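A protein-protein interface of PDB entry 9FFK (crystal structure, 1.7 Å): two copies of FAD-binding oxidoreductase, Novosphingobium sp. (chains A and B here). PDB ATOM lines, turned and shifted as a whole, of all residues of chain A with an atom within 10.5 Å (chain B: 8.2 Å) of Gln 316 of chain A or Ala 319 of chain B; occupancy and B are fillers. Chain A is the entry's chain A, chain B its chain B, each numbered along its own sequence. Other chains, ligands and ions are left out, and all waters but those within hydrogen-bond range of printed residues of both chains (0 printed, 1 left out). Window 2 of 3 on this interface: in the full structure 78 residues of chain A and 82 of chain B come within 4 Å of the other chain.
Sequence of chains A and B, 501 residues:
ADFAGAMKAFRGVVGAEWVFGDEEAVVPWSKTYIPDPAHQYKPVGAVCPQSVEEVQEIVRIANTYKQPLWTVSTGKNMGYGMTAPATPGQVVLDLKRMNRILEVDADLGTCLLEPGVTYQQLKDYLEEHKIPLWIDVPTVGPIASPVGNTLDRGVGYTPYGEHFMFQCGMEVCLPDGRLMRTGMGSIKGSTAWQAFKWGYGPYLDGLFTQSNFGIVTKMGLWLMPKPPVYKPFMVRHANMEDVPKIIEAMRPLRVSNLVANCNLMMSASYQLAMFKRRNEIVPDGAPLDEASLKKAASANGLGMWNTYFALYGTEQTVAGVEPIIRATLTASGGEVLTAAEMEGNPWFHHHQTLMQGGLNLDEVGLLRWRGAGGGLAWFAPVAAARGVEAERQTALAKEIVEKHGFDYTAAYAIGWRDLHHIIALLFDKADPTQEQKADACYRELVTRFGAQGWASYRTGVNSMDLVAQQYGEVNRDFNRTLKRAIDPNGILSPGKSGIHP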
ATOM      1  N   PRO A 228       5.080  12.277   1.334  1.00  0.00           N
ATOM      2  CA  PRO A 228       3.842  13.041   1.135  1.00  0.00           C
ATOM      3  C   PRO A 228       2.637  12.101   1.132  1.00  0.00           C
ATOM      4  O   PRO A 228       1.716  12.362   1.878  1.00  0.00           O
ATOM      5  CB  PRO A 228       4.045  13.681  -0.241  1.00  0.00           C
ATOM      6  CG  PRO A 228       5.556  13.833  -0.366  1.00  0.00           C
ATOM      7  CD  PRO A 228       6.143  12.650   0.387  1.00  0.00           C
ATOM      8  N   VAL A 229       2.739  11.040   0.327  1.00  0.00           N
ATOM      9  CA  VAL A 229       1.664  10.057  -0.004  1.00  0.00           C
ATOM     10  C   VAL A 229       2.101   8.615   0.312  1.00  0.00           C
ATOM     11  O   VAL A 229       3.209   8.196  -0.099  1.00  0.00           O
ATOM     12  CB  VAL A 229       1.230  10.222  -1.475  1.00  0.00           C
ATOM     13  CG1 VAL A 229       0.268   9.126  -1.936  1.00  0.00           C
ATOM     14  CG2 VAL A 229       0.651  11.618  -1.645  1.00  0.00           C
ATOM     15  N   TYR A 230       1.201   7.902   0.990  1.00  0.00           N
ATOM     16  CA  TYR A 230       1.277   6.460   1.337  1.00  0.00           C
ATOM     17  C   TYR A 230       0.052   5.757   0.750  1.00  0.00           C
ATOM     18  O   TYR A 230      -1.076   6.134   1.120  1.00  0.00           O
ATOM     19  CB  TYR A 230       1.219   6.291   2.853  1.00  0.00           C
ATOM     20  CG  TYR A 230       1.013   4.870   3.305  1.00  0.00           C
ATOM     21  CD1 TYR A 230       1.833   3.849   2.857  1.00  0.00           C
ATOM     22  CD2 TYR A 230       0.031   4.549   4.226  1.00  0.00           C
ATOM     23  CE1 TYR A 230       1.675   2.539   3.285  1.00  0.00           C
ATOM     24  CE2 TYR A 230      -0.120   3.250   4.686  1.00  0.00           C
ATOM     25  CZ  TYR A 230       0.698   2.242   4.217  1.00  0.00           C
ATOM     26  OH  TYR A 230       0.470   0.973   4.652  1.00  0.00           O
ATOM     27  N   LYS A 231       0.248   4.741  -0.065  1.00  0.00           N
ATOM     28  CA  LYS A 231      -0.891   4.004  -0.686  1.00  0.00           C
ATOM     29  C   LYS A 231      -0.723   2.509  -0.448  1.00  0.00           C
ATOM     30  O   LYS A 231       0.046   1.832  -1.132  1.00  0.00           O
ATOM     31  CB  LYS A 231      -1.063   4.273  -2.182  1.00  0.00           C
ATOM     32  CG  LYS A 231      -2.411   3.790  -2.710  1.00  0.00           C
ATOM     33  CD  LYS A 231      -2.704   4.197  -4.135  1.00  0.00           C
ATOM     34  CE  LYS A 231      -4.146   3.923  -4.490  1.00  0.00           C
ATOM     35  NZ  LYS A 231      -4.376   4.298  -5.897  1.00  0.00           N
ATOM     36  N   LEU A 311       2.930   1.687  -2.004  1.00  0.00           N
ATOM     37  CA  LEU A 311       3.628   2.728  -2.787  1.00  0.00           C
ATOM     38  C   LEU A 311       3.754   3.972  -1.925  1.00  0.00           C
ATOM     39  O   LEU A 311       2.847   4.232  -1.114  1.00  0.00           O
ATOM     40  CB  LEU A 311       2.813   3.008  -4.055  1.00  0.00           C
ATOM     41  CG  LEU A 311       2.785   1.853  -5.036  1.00  0.00           C
ATOM     42  CD1 LEU A 311       1.981   2.227  -6.273  1.00  0.00           C
ATOM     43  CD2 LEU A 311       4.200   1.417  -5.395  1.00  0.00           C
ATOM     44  N   TYR A 312       4.898   4.654  -2.036  1.00  0.00           N
ATOM     45  CA  TYR A 312       5.255   5.811  -1.203  1.00  0.00           C
ATOM     46  C   TYR A 312       5.786   6.909  -2.113  1.00  0.00           C
ATOM     47  O   TYR A 312       6.562   6.562  -3.025  1.00  0.00           O
ATOM     48  CB  TYR A 312       6.361   5.412  -0.227  1.00  0.00           C
ATOM     49  CG  TYR A 312       6.140   4.122   0.512  1.00  0.00           C
ATOM     50  CD1 TYR A 312       6.461   2.886  -0.042  1.00  0.00           C
ATOM     51  CD2 TYR A 312       5.560   4.138   1.759  1.00  0.00           C
ATOM     52  CE1 TYR A 312       6.248   1.704   0.653  1.00  0.00           C
ATOM     53  CE2 TYR A 312       5.362   2.972   2.473  1.00  0.00           C
ATOM     54  CZ  TYR A 312       5.661   1.754   1.905  1.00  0.00           C
ATOM     55  OH  TYR A 312       5.518   0.617   2.670  1.00  0.00           O
ATOM     56  N   GLY A 313       5.434   8.162  -1.833  1.00  0.00           N
ATOM     57  CA  GLY A 313       5.984   9.336  -2.545  1.00  0.00           C
ATOM     58  C   GLY A 313       4.914  10.388  -2.770  1.00  0.00           C
ATOM     59  O   GLY A 313       4.273  10.810  -1.804  1.00  0.00           O
ATOM     60  N   THR A 314       4.738  10.808  -4.008  1.00  0.00           N
ATOM     61  CA  THR A 314       3.710  11.798  -4.400  1.00  0.00           C
ATOM     62  C   THR A 314       2.596  11.067  -5.133  1.00  0.00           C
ATOM     63  O   THR A 314       2.790   9.894  -5.495  1.00  0.00           O
ATOM     64  CB  THR A 314       4.324  12.887  -5.289  1.00  0.00           C
ATOM     65  OG1 THR A 314       4.778  12.258  -6.495  1.00  0.00           O
ATOM     66  CG2 THR A 314       5.478  13.590  -4.600  1.00  0.00           C
ATOM     67  N   GLU A 315       1.513  11.780  -5.415  1.00  0.00           N
ATOM     68  CA  GLU A 315       0.405  11.240  -6.224  1.00  0.00           C
ATOM     69  C   GLU A 315       1.018  10.923  -7.582  1.00  0.00           C
ATOM     70  O   GLU A 315       0.691   9.872  -8.140  1.00  0.00           O
ATOM     71  CB  GLU A 315      -0.765  12.224  -6.268  1.00  0.00           C
ATOM     72  CG  GLU A 315      -1.372  12.470  -4.895  1.00  0.00           C
ATOM     73  CD  GLU A 315      -0.645  13.487  -4.020  1.00  0.00           C
ATOM     74  OE1 GLU A 315       0.472  13.939  -4.406  1.00  0.00           O
ATOM     75  OE2 GLU A 315      -1.191  13.823  -2.932  1.00  0.00           O
ATOM     76  N   GLN A 316       1.957  11.760  -8.031  1.00  0.00           N
ATOM     77  CA  GLN A 316       2.586  11.619  -9.375  1.00  0.00           C
ATOM     78  C   GLN A 316       3.560  10.430  -9.418  1.00  0.00           C
ATOM     79  O   GLN A 316       3.514   9.686 -10.423  1.00  0.00           O
ATOM     80  CB  GLN A 316       3.226  12.934  -9.824  1.00  0.00           C
ATOM     81  CG  GLN A 316       3.286  13.020 -11.333  1.00  0.00           C
ATOM     82  CD  GLN A 316       3.558  14.394 -11.888  1.00  0.00           C
ATOM     83  OE1 GLN A 316       2.924  15.388 -11.519  1.00  0.00           O
ATOM     84  NE2 GLN A 316       4.462  14.438 -12.851  1.00  0.00           N
ATOM     85  N   THR A 317       4.385  10.189  -8.392  1.00  0.00           N
ATOM     86  CA  THR A 317       5.299   9.007  -8.394  1.00  0.00           C
ATOM     87  C   THR A 317       4.466   7.718  -8.287  1.00  0.00           C
ATOM     88  O   THR A 317       4.794   6.745  -8.995  1.00  0.00           O
ATOM     89  CB  THR A 317       6.407   9.114  -7.336  1.00  0.00           C
ATOM     90  OG1 THR A 317       5.832   9.032  -6.038  1.00  0.00           O
ATOM     91  CG2 THR A 317       7.186  10.405  -7.465  1.00  0.00           C
ATOM     92  N   VAL A 318       3.416   7.709  -7.468  1.00  0.00           N
ATOM     93  CA  VAL A 318       2.496   6.531  -7.349  1.00  0.00           C
ATOM     94  C   VAL A 318       1.890   6.269  -8.743  1.00  0.00           C
ATOM     95  O   VAL A 318       2.030   5.150  -9.244  1.00  0.00           O
ATOM     96  CB  VAL A 318       1.430   6.733  -6.253  1.00  0.00           C
ATOM     97  CG1 VAL A 318       0.359   5.650  -6.265  1.00  0.00           C
ATOM     98  CG2 VAL A 318       2.071   6.840  -4.876  1.00  0.00           C
ATOM     99  N   ALA A 319       1.275   7.276  -9.384  1.00  0.00           N
ATOM    100  CA  ALA A 319       0.636   7.140 -10.722  1.00  0.00           C
ATOM    101  C   ALA A 319       1.632   6.562 -11.747  1.00  0.00           C
ATOM    102  O   ALA A 319       1.206   5.851 -12.675  1.00  0.00           O
ATOM    103  CB  ALA A 319       0.092   8.483 -11.162  1.00  0.00           C
ATOM    104  N   GLY A 320       2.925   6.848 -11.583  1.00  0.00           N
ATOM    105  CA  GLY A 320       4.009   6.366 -12.457  1.00  0.00           C
ATOM    106  C   GLY A 320       4.152   4.849 -12.505  1.00  0.00           C
ATOM    107  O   GLY A 320       4.588   4.356 -13.537  1.00  0.00           O
ATOM    108  N   VAL A 321       3.840   4.117 -11.431  1.00  0.00           N
ATOM    109  CA  VAL A 321       4.159   2.658 -11.361  1.00  0.00           C
ATOM    110  C   VAL A 321       2.902   1.821 -11.112  1.00  0.00           C
ATOM    111  O   VAL A 321       2.948   0.628 -11.421  1.00  0.00           O
ATOM    112  CB  VAL A 321       5.242   2.386 -10.300  1.00  0.00           C
ATOM    113  CG1 VAL A 321       6.589   2.945 -10.741  1.00  0.00           C
ATOM    114  CG2 VAL A 321       4.834   2.945  -8.951  1.00  0.00           C
ATOM    115  N   GLU A 322       1.833   2.406 -10.572  1.00  0.00           N
ATOM    116  CA  GLU A 322       0.640   1.619 -10.153  1.00  0.00           C
ATOM    117  C   GLU A 322       0.073   0.870 -11.351  1.00  0.00           C
ATOM    118  O   GLU A 322      -0.262  -0.294 -11.226  1.00  0.00           O
ATOM    119  CB  GLU A 322      -0.412   2.498  -9.502  1.00  0.00           C
ATOM    120  CG  GLU A 322      -1.671   1.759  -9.138  1.00  0.00           C
ATOM    121  CD  GLU A 322      -2.620   2.574  -8.291  1.00  0.00           C
ATOM    122  OE1 GLU A 322      -2.226   3.636  -7.769  1.00  0.00           O
ATOM    123  OE2 GLU A 322      -3.766   2.141  -8.154  1.00  0.00           O
ATOM    124  N   PRO A 323      -0.065   1.492 -12.547  1.00  0.00           N
ATOM    125  CA  PRO A 323      -0.552   0.756 -13.720  1.00  0.00           C
ATOM    126  C   PRO A 323       0.229  -0.519 -14.075  1.00  0.00           C
ATOM    127  O   PRO A 323      -0.369  -1.566 -14.275  1.00  0.00           O
ATOM    128  CB  PRO A 323      -0.427   1.805 -14.845  1.00  0.00           C
ATOM    129  CG  PRO A 323      -0.613   3.124 -14.106  1.00  0.00           C
ATOM    130  CD  PRO A 323       0.175   2.917 -12.825  1.00  0.00           C
ATOM    131  N   VAL B 229      14.392   4.131 -19.517  1.00  0.00           N
ATOM    132  CA  VAL B 229      14.840   5.539 -19.666  1.00  0.00           C
ATOM    133  C   VAL B 229      15.978   5.842 -18.677  1.00  0.00           C
ATOM    134  O   VAL B 229      15.842   5.545 -17.471  1.00  0.00           O
ATOM    135  CB  VAL B 229      13.619   6.465 -19.500  1.00  0.00           C
ATOM    136  CG1 VAL B 229      14.000   7.923 -19.361  1.00  0.00           C
ATOM    137  CG2 VAL B 229      12.649   6.222 -20.651  1.00  0.00           C
ATOM    138  N   LYS B 231      18.396   9.338 -17.925  1.00  0.00           N
ATOM    139  CA  LYS B 231      18.488  10.806 -18.139  1.00  0.00           C
ATOM    140  C   LYS B 231      19.599  11.364 -17.262  1.00  0.00           C
ATOM    141  O   LYS B 231      19.386  11.597 -16.073  1.00  0.00           O
ATOM    142  CB  LYS B 231      17.179  11.528 -17.841  1.00  0.00           C
ATOM    143  CG  LYS B 231      17.198  12.985 -18.261  1.00  0.00           C
ATOM    144  CD  LYS B 231      15.849  13.655 -18.209  1.00  0.00           C
ATOM    145  CE  LYS B 231      15.801  14.920 -19.034  1.00  0.00           C
ATOM    146  NZ  LYS B 231      14.467  15.564 -18.921  1.00  0.00           N
ATOM    147  N   PHE B 233      22.209  14.269 -15.877  1.00  0.00           N
ATOM    148  CA  PHE B 233      22.154  15.718 -15.597  1.00  0.00           C
ATOM    149  C   PHE B 233      23.510  16.184 -15.113  1.00  0.00           C
ATOM    150  O   PHE B 233      24.259  15.400 -14.449  1.00  0.00           O
ATOM    151  CB  PHE B 233      21.145  16.051 -14.503  1.00  0.00           C
ATOM    152  CG  PHE B 233      19.706  15.776 -14.831  1.00  0.00           C
ATOM    153  CD1 PHE B 233      19.171  14.509 -14.657  1.00  0.00           C
ATOM    154  CD2 PHE B 233      18.896  16.787 -15.332  1.00  0.00           C
ATOM    155  CE1 PHE B 233      17.843  14.262 -14.947  1.00  0.00           C
ATOM    156  CE2 PHE B 233      17.572  16.532 -15.648  1.00  0.00           C
ATOM    157  CZ  PHE B 233      17.043  15.279 -15.437  1.00  0.00           C
ATOM    158  N   LEU B 311      18.653  10.186 -13.521  1.00  0.00           N
ATOM    159  CA  LEU B 311      17.296   9.660 -13.260  1.00  0.00           C
ATOM    160  C   LEU B 311      17.102   8.423 -14.117  1.00  0.00           C
ATOM    161  O   LEU B 311      17.583   8.383 -15.248  1.00  0.00           O
ATOM    162  CB  LEU B 311      16.261  10.752 -13.577  1.00  0.00           C
ATOM    163  CG  LEU B 311      16.240  11.884 -12.563  1.00  0.00           C
ATOM    164  CD1 LEU B 311      15.112  12.862 -12.853  1.00  0.00           C
ATOM    165  CD2 LEU B 311      16.165  11.357 -11.129  1.00  0.00           C
ATOM    166  N   GLY B 313      14.365   5.027 -15.056  1.00  0.00           N
ATOM    167  CA  GLY B 313      13.014   4.437 -15.024  1.00  0.00           C
ATOM    168  C   GLY B 313      12.255   4.725 -16.305  1.00  0.00           C
ATOM    169  O   GLY B 313      12.734   4.332 -17.383  1.00  0.00           O
ATOM    170  N   THR B 314      11.061   5.284 -16.200  1.00  0.00           N
ATOM    171  CA  THR B 314      10.218   5.610 -17.383  1.00  0.00           C
ATOM    172  C   THR B 314      10.193   7.124 -17.573  1.00  0.00           C
ATOM    173  O   THR B 314      10.583   7.856 -16.650  1.00  0.00           O
ATOM    174  CB  THR B 314       8.794   5.051 -17.239  1.00  0.00           C
ATOM    175  OG1 THR B 314       8.184   5.719 -16.133  1.00  0.00           O
ATOM    176  CG2 THR B 314       8.779   3.554 -17.003  1.00  0.00           C
ATOM    177  N   GLU B 315       9.660   7.571 -18.708  1.00  0.00           N
ATOM    178  CA  GLU B 315       9.350   9.004 -18.907  1.00  0.00           C
ATOM    179  C   GLU B 315       8.461   9.464 -17.749  1.00  0.00           C
ATOM    180  O   GLU B 315       8.636  10.578 -17.276  1.00  0.00           O
ATOM    181  CB  GLU B 315       8.709   9.220 -20.278  1.00  0.00           C
ATOM    182  CG  GLU B 315       9.674   8.979 -21.426  1.00  0.00           C
ATOM    183  CD  GLU B 315      10.925   9.848 -21.411  1.00  0.00           C
ATOM    184  OE1 GLU B 315      11.053  10.723 -20.516  1.00  0.00           O
ATOM    185  OE2 GLU B 315      11.780   9.648 -22.293  1.00  0.00           O
ATOM    186  N   GLN B 316       7.549   8.625 -17.271  1.00  0.00           N
ATOM    187  CA  GLN B 316       6.613   9.063 -16.209  1.00  0.00           C
ATOM    188  C   GLN B 316       7.313   9.154 -14.843  1.00  0.00           C
ATOM    189  O   GLN B 316       7.046  10.148 -14.146  1.00  0.00           O
ATOM    190  CB  GLN B 316       5.371   8.174 -16.172  1.00  0.00           C
ATOM    191  CG  GLN B 316       4.184   8.925 -15.603  1.00  0.00           C
ATOM    192  CD  GLN B 316       2.846   8.390 -16.042  1.00  0.00           C
ATOM    193  OE1 GLN B 316       2.729   7.658 -17.029  1.00  0.00           O
ATOM    194  NE2 GLN B 316       1.812   8.794 -15.314  1.00  0.00           N
ATOM    195  N   THR B 317       8.140   8.174 -14.439  1.00  0.00           N
ATOM    196  CA  THR B 317       8.813   8.220 -13.110  1.00  0.00           C
ATOM    197  C   THR B 317       9.784   9.405 -13.122  1.00  0.00           C
ATOM    198  O   THR B 317       9.804  10.159 -12.115  1.00  0.00           O
ATOM    199  CB  THR B 317       9.455   6.886 -12.681  1.00  0.00           C
ATOM    200  OG1 THR B 317      10.574   6.531 -13.492  1.00  0.00           O
ATOM    201  CG2 THR B 317       8.451   5.754 -12.724  1.00  0.00           C
ATOM    202  N   VAL B 318      10.549   9.580 -14.209  1.00  0.00           N
ATOM    203  CA  VAL B 318      11.469  10.754 -14.373  1.00  0.00           C
ATOM    204  C   VAL B 318      10.663  12.068 -14.195  1.00  0.00           C
ATOM    205  O   VAL B 318      11.009  12.883 -13.307  1.00  0.00           O
ATOM    206  CB  VAL B 318      12.226  10.700 -15.711  1.00  0.00           C
ATOM    207  CG1 VAL B 318      12.996  11.989 -15.989  1.00  0.00           C
ATOM    208  CG2 VAL B 318      13.144   9.493 -15.779  1.00  0.00           C
ATOM    209  N   ALA B 319       9.583  12.253 -14.961  1.00  0.00           N
ATOM    210  CA  ALA B 319       8.693  13.440 -14.887  1.00  0.00           C
ATOM    211  C   ALA B 319       8.182  13.638 -13.451  1.00  0.00           C
ATOM    212  O   ALA B 319       8.047  14.789 -13.038  1.00  0.00           O
ATOM    213  CB  ALA B 319       7.564  13.278 -15.883  1.00  0.00           C
ATOM    214  N   GLY B 320       7.927  12.563 -12.696  1.00  0.00           N
ATOM    215  CA  GLY B 320       7.531  12.635 -11.269  1.00  0.00           C
ATOM    216  C   GLY B 320       8.519  13.380 -10.368  1.00  0.00           C
ATOM    217  O   GLY B 320       8.092  13.993  -9.388  1.00  0.00           O
ATOM    218  N   VAL B 321       9.821  13.322 -10.622  1.00  0.00           N
ATOM    219  CA  VAL B 321      10.778  13.871  -9.616  1.00  0.00           C
ATOM    220  C   VAL B 321      11.618  15.005 -10.195  1.00  0.00           C
ATOM    221  O   VAL B 321      12.180  15.779  -9.378  1.00  0.00           O
ATOM    222  CB  VAL B 321      11.652  12.753  -9.030  1.00  0.00           C
ATOM    223  CG1 VAL B 321      10.829  11.821  -8.147  1.00  0.00           C
ATOM    224  CG2 VAL B 321      12.364  11.988 -10.127  1.00  0.00           C
ATOM    225  N   GLU B 322      11.705  15.119 -11.519  1.00  0.00           N
ATOM    226  CA  GLU B 322      12.635  16.090 -12.160  1.00  0.00           C
ATOM    227  C   GLU B 322      12.275  17.523 -11.749  1.00  0.00           C
ATOM    228  O   GLU B 322      13.149  18.296 -11.384  1.00  0.00           O
ATOM    229  CB  GLU B 322      12.677  15.924 -13.679  1.00  0.00           C
ATOM    230  CG  GLU B 322      13.662  16.871 -14.322  1.00  0.00           C
ATOM    231  CD  GLU B 322      13.816  16.698 -15.813  1.00  0.00           C
ATOM    232  OE1 GLU B 322      13.455  15.610 -16.348  1.00  0.00           O
ATOM    233  OE2 GLU B 322      14.310  17.636 -16.434  1.00  0.00           O
ATOM    234  N   PRO B 323      10.997  17.940 -11.753  1.00  0.00           N
ATOM    235  CA  PRO B 323      10.656  19.280 -11.280  1.00  0.00           C
ATOM    236  C   PRO B 323      11.130  19.626  -9.866  1.00  0.00           C
ATOM    237  O   PRO B 323      11.707  20.677  -9.716  1.00  0.00           O
ATOM    238  CB  PRO B 323       9.113  19.294 -11.328  1.00  0.00           C
ATOM    239  CG  PRO B 323       8.791  18.294 -12.428  1.00  0.00           C
ATOM    240  CD  PRO B 323       9.825  17.191 -12.237  1.00  0.00           C
ATOM    241  N   ILE B 324      10.886  18.771  -8.863  1.00  0.00           N
ATOM    242  CA  ILE B 324      11.336  19.073  -7.470  1.00  0.00           C
ATOM    243  C   ILE B 324      12.881  19.179  -7.462  1.00  0.00           C
ATOM    244  O   ILE B 324      13.423  20.075  -6.806  1.00  0.00           O
ATOM    245  CB  ILE B 324      10.834  18.027  -6.445  1.00  0.00           C
ATOM    246  CG1 ILE B 324       9.356  17.674  -6.630  1.00  0.00           C
ATOM    247  CG2 ILE B 324      11.116  18.514  -5.031  1.00  0.00           C
ATOM    248  CD1 ILE B 324       8.760  16.878  -5.491  1.00  0.00           C
ATOM    249  N   ILE B 325      13.572  18.304  -8.195  1.00  0.00           N
ATOM    250  CA  ILE B 325      15.066  18.265  -8.246  1.00  0.00           C
ATOM    251  C   ILE B 325      15.578  19.585  -8.840  1.00  0.00           C
ATOM    252  O   ILE B 325      16.458  20.239  -8.221  1.00  0.00           O
ATOM    253  CB  ILE B 325      15.539  17.018  -9.011  1.00  0.00           C
ATOM    254  CG1 ILE B 325      15.217  15.767  -8.185  1.00  0.00           C
ATOM    255  CG2 ILE B 325      17.015  17.102  -9.378  1.00  0.00           C
ATOM    256  CD1 ILE B 325      15.237  14.482  -8.958  1.00  0.00           C
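OG1 of Thr 314 of chain B lies within hydrogen-bond range of N of Thr 317 of chain B.
The side-chain hydroxyl of Thr 314 of chain B sits close to the backbone NH of Gln 316 of chain B (3.2 Å).
The side-chain hydroxyl (OG1) of Thr 314 of chain A sits close to the backbone NH (N) of Gln 316 of chain A (3.3 Å).
The side-chain hydroxyl (OG1) of Thr 314 of chain A sits at hydrogen-bond distance from the backbone NH (N) of Thr 317 of chain A, 2.8 Å away.
Gln 316 of chain A touches Ala 319 of chain B (NE2 to O, 3.6 Å).
Gln 316 of chain A touches Gly 320 of chain B (NE2 to CA, 3.9 Å).
Thr 317 of chain A touches Val 321 of chain B.
Gln 316 of chain B touches Ala 319 of chain A.
Thr 317 of chain B touches Val 321 of chain A.
Gln 316 of chain A touches just these residues of chain B: Ala 319 (3.6 Å) and Gly 320 (3.9 Å).
Of chain A, only Gln 316 (3.6 Å) comes within 4 Å of Ala 319 of chain B.
Gly 320 of chain B touches one residue of chain A.
Of the printed residues of chain B, Val 321 of chain A touches Thr 317.
Of the printed residues of chain A, Gln 316 of chain B touches Ala 319 (3.999 Å).
Printed residues of chain A within 4 Å of Thr 317 of chain B: Val 321 (3.9 Å).
Of the printed residues of chain B, Ala 319 of chain A touches Gln 316.
Tyr 312 of chain A touches none of the printed residues of chain B.
Glu 322 of chain A touches none of the printed residues of chain B.
The nearest residue of chain A that does not touch Ala 319 of chain B is Thr 317 of chain A (6.9 Å).
The nearest printed residue of chain A that does not touch Thr 317 of chain B is Gly 320 of chain A (4.2 Å).
Of the 17 printed residues of chain B, 5 touch a printed residue of chain A.
Of the 17 printed residues of chain A, 4 touch a printed residue of chain B.
Hydrophobic or aromatic side chains of chain A within 4 Å of the printed part of chain B: Val 321.
Among the printed residues, 5 pairs touch across the chains.
Among the printed residues, no Asp or Glu carboxylate lies within 4 Å of a Lys or Arg side-chain nitrogen of the other chain.
Gln 316 of chain A touches Ala 319 of chain B, and with the chains exchanged Ala 319 of chain A touches Gln 316 of chain B.
Gln 316 of chain A touches Gly 320 of chain B, but with the chains exchanged Gly 320 of chain A does not touch Gln 316 of chain B (4.1 Å).
Thr 317 of chain A touches Val 321 of chain B, and with the chains exchanged Val 321 of chain A touches Thr 317 of chain B.
14 positions are printed for both chains.
Of the 5 pairs that touch across the chains among the printed residues, 4 have their exchanged pair printed and touching as well.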
